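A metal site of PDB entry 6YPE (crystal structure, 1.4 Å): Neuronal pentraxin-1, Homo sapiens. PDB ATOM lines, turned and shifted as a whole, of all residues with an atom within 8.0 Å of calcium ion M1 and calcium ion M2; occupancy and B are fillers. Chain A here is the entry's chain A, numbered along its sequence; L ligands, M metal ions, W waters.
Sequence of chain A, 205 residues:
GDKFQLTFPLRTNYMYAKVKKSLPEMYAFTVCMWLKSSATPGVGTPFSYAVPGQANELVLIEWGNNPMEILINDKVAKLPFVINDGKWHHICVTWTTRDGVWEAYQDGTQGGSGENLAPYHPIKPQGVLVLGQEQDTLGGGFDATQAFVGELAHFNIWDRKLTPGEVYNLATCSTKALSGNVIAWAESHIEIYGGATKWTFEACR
The backbone NH of Asp 74 sits at hydrogen-bond distance from the backbone carbonyl oxygen of Asn 56 (2.9 Å).
OG of Ser 48 is in hydrogen-bond range of NE2 of Gln 135 (3.1 Å).
The backbone carbonyl oxygen (O) of Gln 146 is in hydrogen-bond range of the side-chain hydroxyl (OG1) of Thr 45 (2.8 Å).
The side-chain amide oxygen (OE1) of Gln 54 sits at hydrogen-bond distance from the backbone NH (N) of Asn 56, at 2.9 Å.
N of Asp 136 sits at hydrogen-bond distance from O of Gly 141 (3.3 Å).
The nearest printed residue that does not touch calcium ion M1 is Ala 55 (4.5 Å).
O1 of the ligand binds calcium ion M2, at 2.2 Å.
Calcium ion M2 is bound by OE2 of Glu 134, 2.3 Å away.
OE1 of Gln 146 is bound to calcium ion M2 (2.4 Å).
Water W3 is bound to calcium ion M2, at 2.4 Å.
Water W2 binds calcium ion M2.
OD2 of Asp 136 is bound to calcium ion M2.
The side-chain carboxylate (OD1) of Asp 136 binds calcium ion M2 (2.6 Å).
Calcium ion M1 is bound by the backbone carbonyl oxygen (O) of Gln 135 (2.3 Å), the side-chain amide oxygen (OD1) of Asn 56 (2.3 Å), an oxygen (O2) of the ligand (2.3 Å), the side-chain carboxylate (OE1) of Glu 134 (2.4 Å), the side-chain carboxylate (OD1) of Asp 136 (2.4 Å), water W1 (2.4 Å) and the side-chain carboxylate (OE2) of Glu 134 (2.6 Å).
Calcium ion M1 has seven donor atoms within binding distance.
Three residues have an atom within 4 Å of calcium ion M2: Glu 134, Asp 136 and Gln 146.
Water W2 lies within hydrogen-bond range of O of Gly 141, O of Glu 134 and N of Asp 143.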
ATOM      1  N   THR A  45      13.739  -2.297  20.433  1.00  0.00           N
ATOM      2  CA  THR A  45      13.854  -3.635  19.858  1.00  0.00           C
ATOM      3  C   THR A  45      15.150  -4.323  20.264  1.00  0.00           C
ATOM      4  O   THR A  45      16.186  -4.143  19.601  1.00  0.00           O
ATOM      5  CB  THR A  45      13.764  -3.555  18.336  1.00  0.00           C
ATOM      6  OG1 THR A  45      12.543  -2.900  17.966  1.00  0.00           O
ATOM      7  CG2 THR A  45      13.762  -4.934  17.710  1.00  0.00           C
ATOM      8  N   SER A  48      15.875  -8.573  16.422  1.00  0.00           N
ATOM      9  CA  SER A  48      14.969  -8.936  15.346  1.00  0.00           C
ATOM     10  C   SER A  48      15.664  -9.907  14.403  1.00  0.00           C
ATOM     11  O   SER A  48      16.900  -9.964  14.334  1.00  0.00           O
ATOM     12  CB  SER A  48      14.483  -7.707  14.579  1.00  0.00           C
ATOM     13  OG  SER A  48      15.566  -7.054  13.923  1.00  0.00           O
ATOM     14  N   TYR A  49      14.843 -10.673  13.698  1.00  0.00           N
ATOM     15  CA  TYR A  49      15.294 -11.711  12.788  1.00  0.00           C
ATOM     16  C   TYR A  49      14.434 -11.672  11.539  1.00  0.00           C
ATOM     17  O   TYR A  49      13.207 -11.787  11.633  1.00  0.00           O
ATOM     18  CB  TYR A  49      15.177 -13.078  13.471  1.00  0.00           C
ATOM     19  CG  TYR A  49      15.507 -14.247  12.582  1.00  0.00           C
ATOM     20  CD1 TYR A  49      16.826 -14.492  12.177  1.00  0.00           C
ATOM     21  CD2 TYR A  49      14.520 -15.138  12.178  1.00  0.00           C
ATOM     22  CE1 TYR A  49      17.129 -15.570  11.384  1.00  0.00           C
ATOM     23  CE2 TYR A  49      14.818 -16.227  11.376  1.00  0.00           C
ATOM     24  CZ  TYR A  49      16.133 -16.442  10.985  1.00  0.00           C
ATOM     25  OH  TYR A  49      16.422 -17.519  10.196  1.00  0.00           O
ATOM     26  N   ALA A  50      15.077 -11.440  10.393  1.00  0.00           N
ATOM     27  CA  ALA A  50      14.438 -11.306   9.099  1.00  0.00           C
ATOM     28  C   ALA A  50      14.866 -12.427   8.164  1.00  0.00           C
ATOM     29  O   ALA A  50      16.032 -12.808   8.141  1.00  0.00           O
ATOM     30  CB  ALA A  50      14.879  -9.983   8.470  1.00  0.00           C
ATOM     31  N   GLN A  54       9.995 -12.070   4.704  1.00  0.00           N
ATOM     32  CA  GLN A  54       9.383 -11.724   5.990  1.00  0.00           C
ATOM     33  C   GLN A  54      10.453 -11.116   6.894  1.00  0.00           C
ATOM     34  O   GLN A  54      11.192 -11.844   7.569  1.00  0.00           O
ATOM     35  CB  GLN A  54       8.732 -12.939   6.636  1.00  0.00           C
ATOM     36  CG  GLN A  54       8.104 -12.633   7.984  1.00  0.00           C
ATOM     37  CD  GLN A  54       7.098 -11.504   7.919  1.00  0.00           C
ATOM     38  OE1 GLN A  54       7.423 -10.351   8.218  1.00  0.00           O
ATOM     39  NE2 GLN A  54       5.860 -11.821   7.550  1.00  0.00           N
ATOM     40  N   ALA A  55      10.514  -9.795   6.927  1.00  0.00           N
ATOM     41  CA  ALA A  55      11.477  -9.130   7.782  1.00  0.00           C
ATOM     42  C   ALA A  55      11.125  -9.202   9.255  1.00  0.00           C
ATOM     43  O   ALA A  55      11.986  -8.912  10.092  1.00  0.00           O
ATOM     44  CB  ALA A  55      11.621  -7.670   7.384  1.00  0.00           C
ATOM     45  N   ASN A  56       9.879  -9.568   9.591  1.00  0.00           N
ATOM     46  CA  ASN A  56       9.442  -9.687  10.977  1.00  0.00           C
ATOM     47  C   ASN A  56       9.263 -11.157  11.347  1.00  0.00           C
ATOM     48  O   ASN A  56       8.248 -11.538  11.927  1.00  0.00           O
ATOM     49  CB  ASN A  56       8.121  -8.961  11.207  1.00  0.00           C
ATOM     50  CG  ASN A  56       8.213  -7.461  10.986  1.00  0.00           C
ATOM     51  OD1 ASN A  56       9.284  -6.912  10.710  1.00  0.00           O
ATOM     52  ND2 ASN A  56       7.072  -6.788  11.106  1.00  0.00           N
ATOM     53  N   GLU A  57      10.250 -11.995  11.026  1.00  0.00           N
ATOM     54  CA  GLU A  57      10.100 -13.425  11.264  1.00  0.00           C
ATOM     55  C   GLU A  57      10.161 -13.746  12.760  1.00  0.00           C
ATOM     56  O   GLU A  57       9.388 -14.586  13.245  1.00  0.00           O
ATOM     57  CB  GLU A  57      11.153 -14.214  10.467  1.00  0.00           C
ATOM     58  CG  GLU A  57      11.115 -15.710  10.626  1.00  0.00           C
ATOM     59  CD  GLU A  57       9.834 -16.355  10.107  1.00  0.00           C
ATOM     60  OE1 GLU A  57       8.979 -15.656   9.525  1.00  0.00           O
ATOM     61  OE2 GLU A  57       9.700 -17.581  10.290  1.00  0.00           O
ATOM     62  N   VAL A  59      10.762 -11.190  16.306  1.00  0.00           N
ATOM     63  CA  VAL A  59      11.040  -9.840  16.784  1.00  0.00           C
ATOM     64  C   VAL A  59      10.586  -9.711  18.237  1.00  0.00           C
ATOM     65  O   VAL A  59       9.520 -10.211  18.607  1.00  0.00           O
ATOM     66  CB  VAL A  59      10.293  -8.772  15.961  1.00  0.00           C
ATOM     67  CG1 VAL A  59      10.835  -7.372  16.279  1.00  0.00           C
ATOM     68  CG2 VAL A  59      10.375  -9.054  14.481  1.00  0.00           C
ATOM     69  N   ILE A  61       9.918  -6.429  20.713  1.00  0.00           N
ATOM     70  CA  ILE A  61       9.799  -4.985  20.504  1.00  0.00           C
ATOM     71  C   ILE A  61       8.807  -4.371  21.472  1.00  0.00           C
ATOM     72  O   ILE A  61       7.686  -4.867  21.645  1.00  0.00           O
ATOM     73  CB  ILE A  61       9.427  -4.638  19.043  1.00  0.00           C
ATOM     74  CG1 ILE A  61       9.277  -3.131  18.906  1.00  0.00           C
ATOM     75  CG2 ILE A  61       8.144  -5.314  18.618  1.00  0.00           C
ATOM     76  CD1 ILE A  61       9.241  -2.646  17.465  1.00  0.00           C
ATOM     77  N   TRP A  63       7.425  -0.656  21.344  1.00  0.00           N
ATOM     78  CA  TRP A  63       7.544   0.483  20.439  1.00  0.00           C
ATOM     79  C   TRP A  63       6.650   1.610  20.920  1.00  0.00           C
ATOM     80  O   TRP A  63       5.422   1.530  20.804  1.00  0.00           O
ATOM     81  CB  TRP A  63       7.175   0.065  19.019  1.00  0.00           C
ATOM     82  CG  TRP A  63       7.340   1.124  17.944  1.00  0.00           C
ATOM     83  CD1 TRP A  63       8.101   2.262  17.980  1.00  0.00           C
ATOM     84  CD2 TRP A  63       6.717   1.102  16.661  1.00  0.00           C
ATOM     85  NE1 TRP A  63       7.993   2.946  16.791  1.00  0.00           N
ATOM     86  CE2 TRP A  63       7.162   2.250  15.962  1.00  0.00           C
ATOM     87  CE3 TRP A  63       5.850   0.219  16.013  1.00  0.00           C
ATOM     88  CZ2 TRP A  63       6.732   2.539  14.663  1.00  0.00           C
ATOM     89  CZ3 TRP A  63       5.432   0.500  14.731  1.00  0.00           C
ATOM     90  CH2 TRP A  63       5.881   1.652  14.061  1.00  0.00           C
ATOM     91  N   LEU A  71       6.876 -10.949  18.070  1.00  0.00           N
ATOM     92  CA  LEU A  71       6.304 -11.215  16.755  1.00  0.00           C
ATOM     93  C   LEU A  71       6.959 -12.471  16.201  1.00  0.00           C
ATOM     94  O   LEU A  71       8.183 -12.601  16.260  1.00  0.00           O
ATOM     95  CB  LEU A  71       6.550 -10.091  15.745  1.00  0.00           C
ATOM     96  CG  LEU A  71       6.406  -8.642  16.142  1.00  0.00           C
ATOM     97  CD1 LEU A  71       6.619  -7.746  14.918  1.00  0.00           C
ATOM     98  CD2 LEU A  71       5.065  -8.460  16.644  1.00  0.00           C
ATOM     99  N   ASP A  74       5.381 -12.110  11.750  1.00  0.00           N
ATOM    100  CA  ASP A  74       4.585 -10.893  11.781  1.00  0.00           C
ATOM    101  C   ASP A  74       3.240 -11.076  12.493  1.00  0.00           C
ATOM    102  O   ASP A  74       2.283 -10.349  12.208  1.00  0.00           O
ATOM    103  CB  ASP A  74       4.382 -10.285  10.387  1.00  0.00           C
ATOM    104  CG  ASP A  74       3.955  -8.839  10.443  1.00  0.00           C
ATOM    105  OD1 ASP A  74       4.450  -8.093  11.331  1.00  0.00           O
ATOM    106  OD2 ASP A  74       3.130  -8.437   9.602  1.00  0.00           O
ATOM    107  N   GLN A 133      17.992  -3.279  16.807  1.00  0.00           N
ATOM    108  CA  GLN A 133      17.193  -2.618  15.783  1.00  0.00           C
ATOM    109  C   GLN A 133      16.153  -3.584  15.246  1.00  0.00           C
ATOM    110  O   GLN A 133      16.328  -4.810  15.271  1.00  0.00           O
ATOM    111  CB  GLN A 133      18.041  -2.165  14.595  1.00  0.00           C
ATOM    112  CG  GLN A 133      19.159  -1.177  14.894  1.00  0.00           C
ATOM    113  CD  GLN A 133      18.673   0.251  15.133  1.00  0.00           C
ATOM    114  OE1 GLN A 133      17.551   0.618  14.776  1.00  0.00           O
ATOM    115  NE2 GLN A 133      19.526   1.062  15.735  1.00  0.00           N
ATOM    116  N   GLU A 134      15.076  -3.003  14.717  1.00  0.00           N
ATOM    117  CA  GLU A 134      13.993  -3.698  14.034  1.00  0.00           C
ATOM    118  C   GLU A 134      14.246  -3.618  12.534  1.00  0.00           C
ATOM    119  O   GLU A 134      14.635  -2.565  12.019  1.00  0.00           O
ATOM    120  CB  GLU A 134      12.678  -2.976  14.365  1.00  0.00           C
ATOM    121  CG  GLU A 134      11.396  -3.816  14.279  1.00  0.00           C
ATOM    122  CD  GLU A 134      10.876  -4.035  12.873  1.00  0.00           C
ATOM    123  OE1 GLU A 134      10.339  -5.132  12.612  1.00  0.00           O
ATOM    124  OE2 GLU A 134      10.972  -3.112  12.030  1.00  0.00           O
ATOM    125  N   GLN A 135      14.049  -4.742  11.834  1.00  0.00           N
ATOM    126  CA  GLN A 135      14.355  -4.832  10.417  1.00  0.00           C
ATOM    127  C   GLN A 135      13.107  -4.662   9.548  1.00  0.00           C
ATOM    128  O   GLN A 135      12.058  -5.240   9.835  1.00  0.00           O
ATOM    129  CB  GLN A 135      15.016  -6.168  10.088  1.00  0.00           C
ATOM    130  CG  GLN A 135      16.428  -6.281  10.599  1.00  0.00           C
ATOM    131  CD  GLN A 135      16.993  -7.680  10.461  1.00  0.00           C
ATOM    132  OE1 GLN A 135      17.506  -8.073   9.408  1.00  0.00           O
ATOM    133  NE2 GLN A 135      16.893  -8.446  11.533  1.00  0.00           N
ATOM    134  N   ASP A 136      13.242  -3.857   8.489  1.00  0.00           N
ATOM    135  CA  ASP A 136      12.230  -3.767   7.449  1.00  0.00           C
ATOM    136  C   ASP A 136      12.731  -4.314   6.122  1.00  0.00           C
ATOM    137  O   ASP A 136      11.929  -4.478   5.194  1.00  0.00           O
ATOM    138  CB  ASP A 136      11.729  -2.318   7.297  1.00  0.00           C
ATOM    139  CG  ASP A 136      10.982  -1.828   8.521  1.00  0.00           C
ATOM    140  OD1 ASP A 136      10.479  -2.685   9.280  1.00  0.00           O
ATOM    141  OD2 ASP A 136      10.909  -0.605   8.738  1.00  0.00           O
ATOM    142  N   THR A 137      14.031  -4.618   6.030  1.00  0.00           N
ATOM    143  CA  THR A 137      14.606  -5.331   4.905  1.00  0.00           C
ATOM    144  C   THR A 137      15.532  -6.396   5.480  1.00  0.00           C
ATOM    145  O   THR A 137      15.812  -6.419   6.677  1.00  0.00           O
ATOM    146  CB  THR A 137      15.413  -4.397   4.001  1.00  0.00           C
ATOM    147  OG1 THR A 137      16.558  -3.920   4.711  1.00  0.00           O
ATOM    148  CG2 THR A 137      14.591  -3.186   3.581  1.00  0.00           C
ATOM    149  N   GLY A 140      18.491  -4.959   7.383  1.00  0.00           N
ATOM    150  CA  GLY A 140      18.516  -3.507   7.402  1.00  0.00           C
ATOM    151  C   GLY A 140      17.142  -2.872   7.485  1.00  0.00           C
ATOM    152  O   GLY A 140      16.199  -3.459   8.009  1.00  0.00           O
ATOM    153  N   GLY A 141      17.016  -1.663   6.944  1.00  0.00           N
ATOM    154  CA  GLY A 141      15.770  -0.940   7.022  1.00  0.00           C
ATOM    155  C   GLY A 141      15.404  -0.557   8.448  1.00  0.00           C
ATOM    156  O   GLY A 141      14.264  -0.751   8.868  1.00  0.00           O
ATOM    157  N   PHE A 142      16.360   0.001   9.187  1.00  0.00           N
ATOM    158  CA  PHE A 142      16.191   0.332  10.592  1.00  0.00           C
ATOM    159  C   PHE A 142      15.427   1.655  10.787  1.00  0.00           C
ATOM    160  O   PHE A 142      15.461   2.567   9.946  1.00  0.00           O
ATOM    161  CB  PHE A 142      17.551   0.428  11.280  1.00  0.00           C
ATOM    162  CG  PHE A 142      18.399  -0.795  11.165  1.00  0.00           C
ATOM    163  CD1 PHE A 142      17.855  -2.073  11.098  1.00  0.00           C
ATOM    164  CD2 PHE A 142      19.788  -0.695  11.146  1.00  0.00           C
ATOM    165  CE1 PHE A 142      18.666  -3.202  11.005  1.00  0.00           C
ATOM    166  CE2 PHE A 142      20.590  -1.805  11.058  1.00  0.00           C
ATOM    167  CZ  PHE A 142      20.026  -3.067  10.994  1.00  0.00           C
ATOM    168  N   ASP A 143      14.800   1.766  11.956  1.00  0.00           N
ATOM    169  CA  ASP A 143      13.942   2.884  12.328  1.00  0.00           C
ATOM    170  C   ASP A 143      14.336   3.303  13.731  1.00  0.00           C
ATOM    171  O   ASP A 143      14.165   2.543  14.689  1.00  0.00           O
ATOM    172  CB  ASP A 143      12.472   2.424  12.298  1.00  0.00           C
ATOM    173  CG  ASP A 143      11.493   3.515  12.727  1.00  0.00           C
ATOM    174  OD1 ASP A 143      11.896   4.527  13.316  1.00  0.00           O
ATOM    175  OD2 ASP A 143      10.282   3.301  12.493  1.00  0.00           O
ATOM    176  N   ALA A 144      14.886   4.519  13.865  1.00  0.00           N
ATOM    177  CA  ALA A 144      15.375   4.971  15.156  1.00  0.00           C
ATOM    178  C   ALA A 144      14.301   4.951  16.228  1.00  0.00           C
ATOM    179  O   ALA A 144      14.602   4.748  17.401  1.00  0.00           O
ATOM    180  CB  ALA A 144      15.985   6.371  15.048  1.00  0.00           C
ATOM    181  N   THR A 145      13.026   5.169  15.857  1.00  0.00           N
ATOM    182  CA  THR A 145      11.991   5.178  16.892  1.00  0.00           C
ATOM    183  C   THR A 145      11.763   3.799  17.482  1.00  0.00           C
ATOM    184  O   THR A 145      11.150   3.699  18.562  1.00  0.00           O
ATOM    185  CB  THR A 145      10.662   5.741  16.373  1.00  0.00           C
ATOM    186  OG1 THR A 145      10.025   4.786  15.509  1.00  0.00           O
ATOM    187  CG2 THR A 145      10.884   7.049  15.630  1.00  0.00           C
ATOM    188  N   GLN A 146      12.231   2.745  16.820  1.00  0.00           N
ATOM    189  CA  GLN A 146      12.119   1.366  17.267  1.00  0.00           C
ATOM    190  C   GLN A 146      13.415   0.842  17.866  1.00  0.00           C
ATOM    191  O   GLN A 146      13.441  -0.293  18.345  1.00  0.00           O
ATOM    192  CB  GLN A 146      11.701   0.474  16.092  1.00  0.00           C
ATOM    193  CG  GLN A 146      10.309   0.796  15.555  1.00  0.00           C
ATOM    194  CD  GLN A 146       9.925  -0.001  14.321  1.00  0.00           C
ATOM    195  OE1 GLN A 146      10.737  -0.207  13.417  1.00  0.00           O
ATOM    196  NE2 GLN A 146       8.674  -0.412  14.260  1.00  0.00           N
HETATM  197 AS1  LIG L   1       7.174  -2.746  11.622  1.00  0.00          AS
HETATM  198  O1  LIG L   1       8.328  -1.437  11.588  1.00  0.00           O
HETATM  199  O2  LIG L   1       7.686  -4.068  10.617  1.00  0.00           O
HETATM  200  C1  LIG L   1       7.094  -3.473  13.453  1.00  0.00           C
HETATM  201  C2  LIG L   1       5.392  -2.093  11.089  1.00  0.00           C
HETATM  202 CA    CA M   1       9.886  -4.716  10.337  1.00  0.00          CA
HETATM  203 CA    CA M   2      10.451  -1.016  11.209  1.00  0.00          CA
HETATM  204  O   HOH W   1       8.973  -5.270   8.211  1.00  0.00           O
HETATM  205  O   HOH W   2      12.849  -0.789  11.098  1.00  0.00           O
HETATM  206  O   HOH W   3       9.714   1.235  10.857  1.00  0.00           O
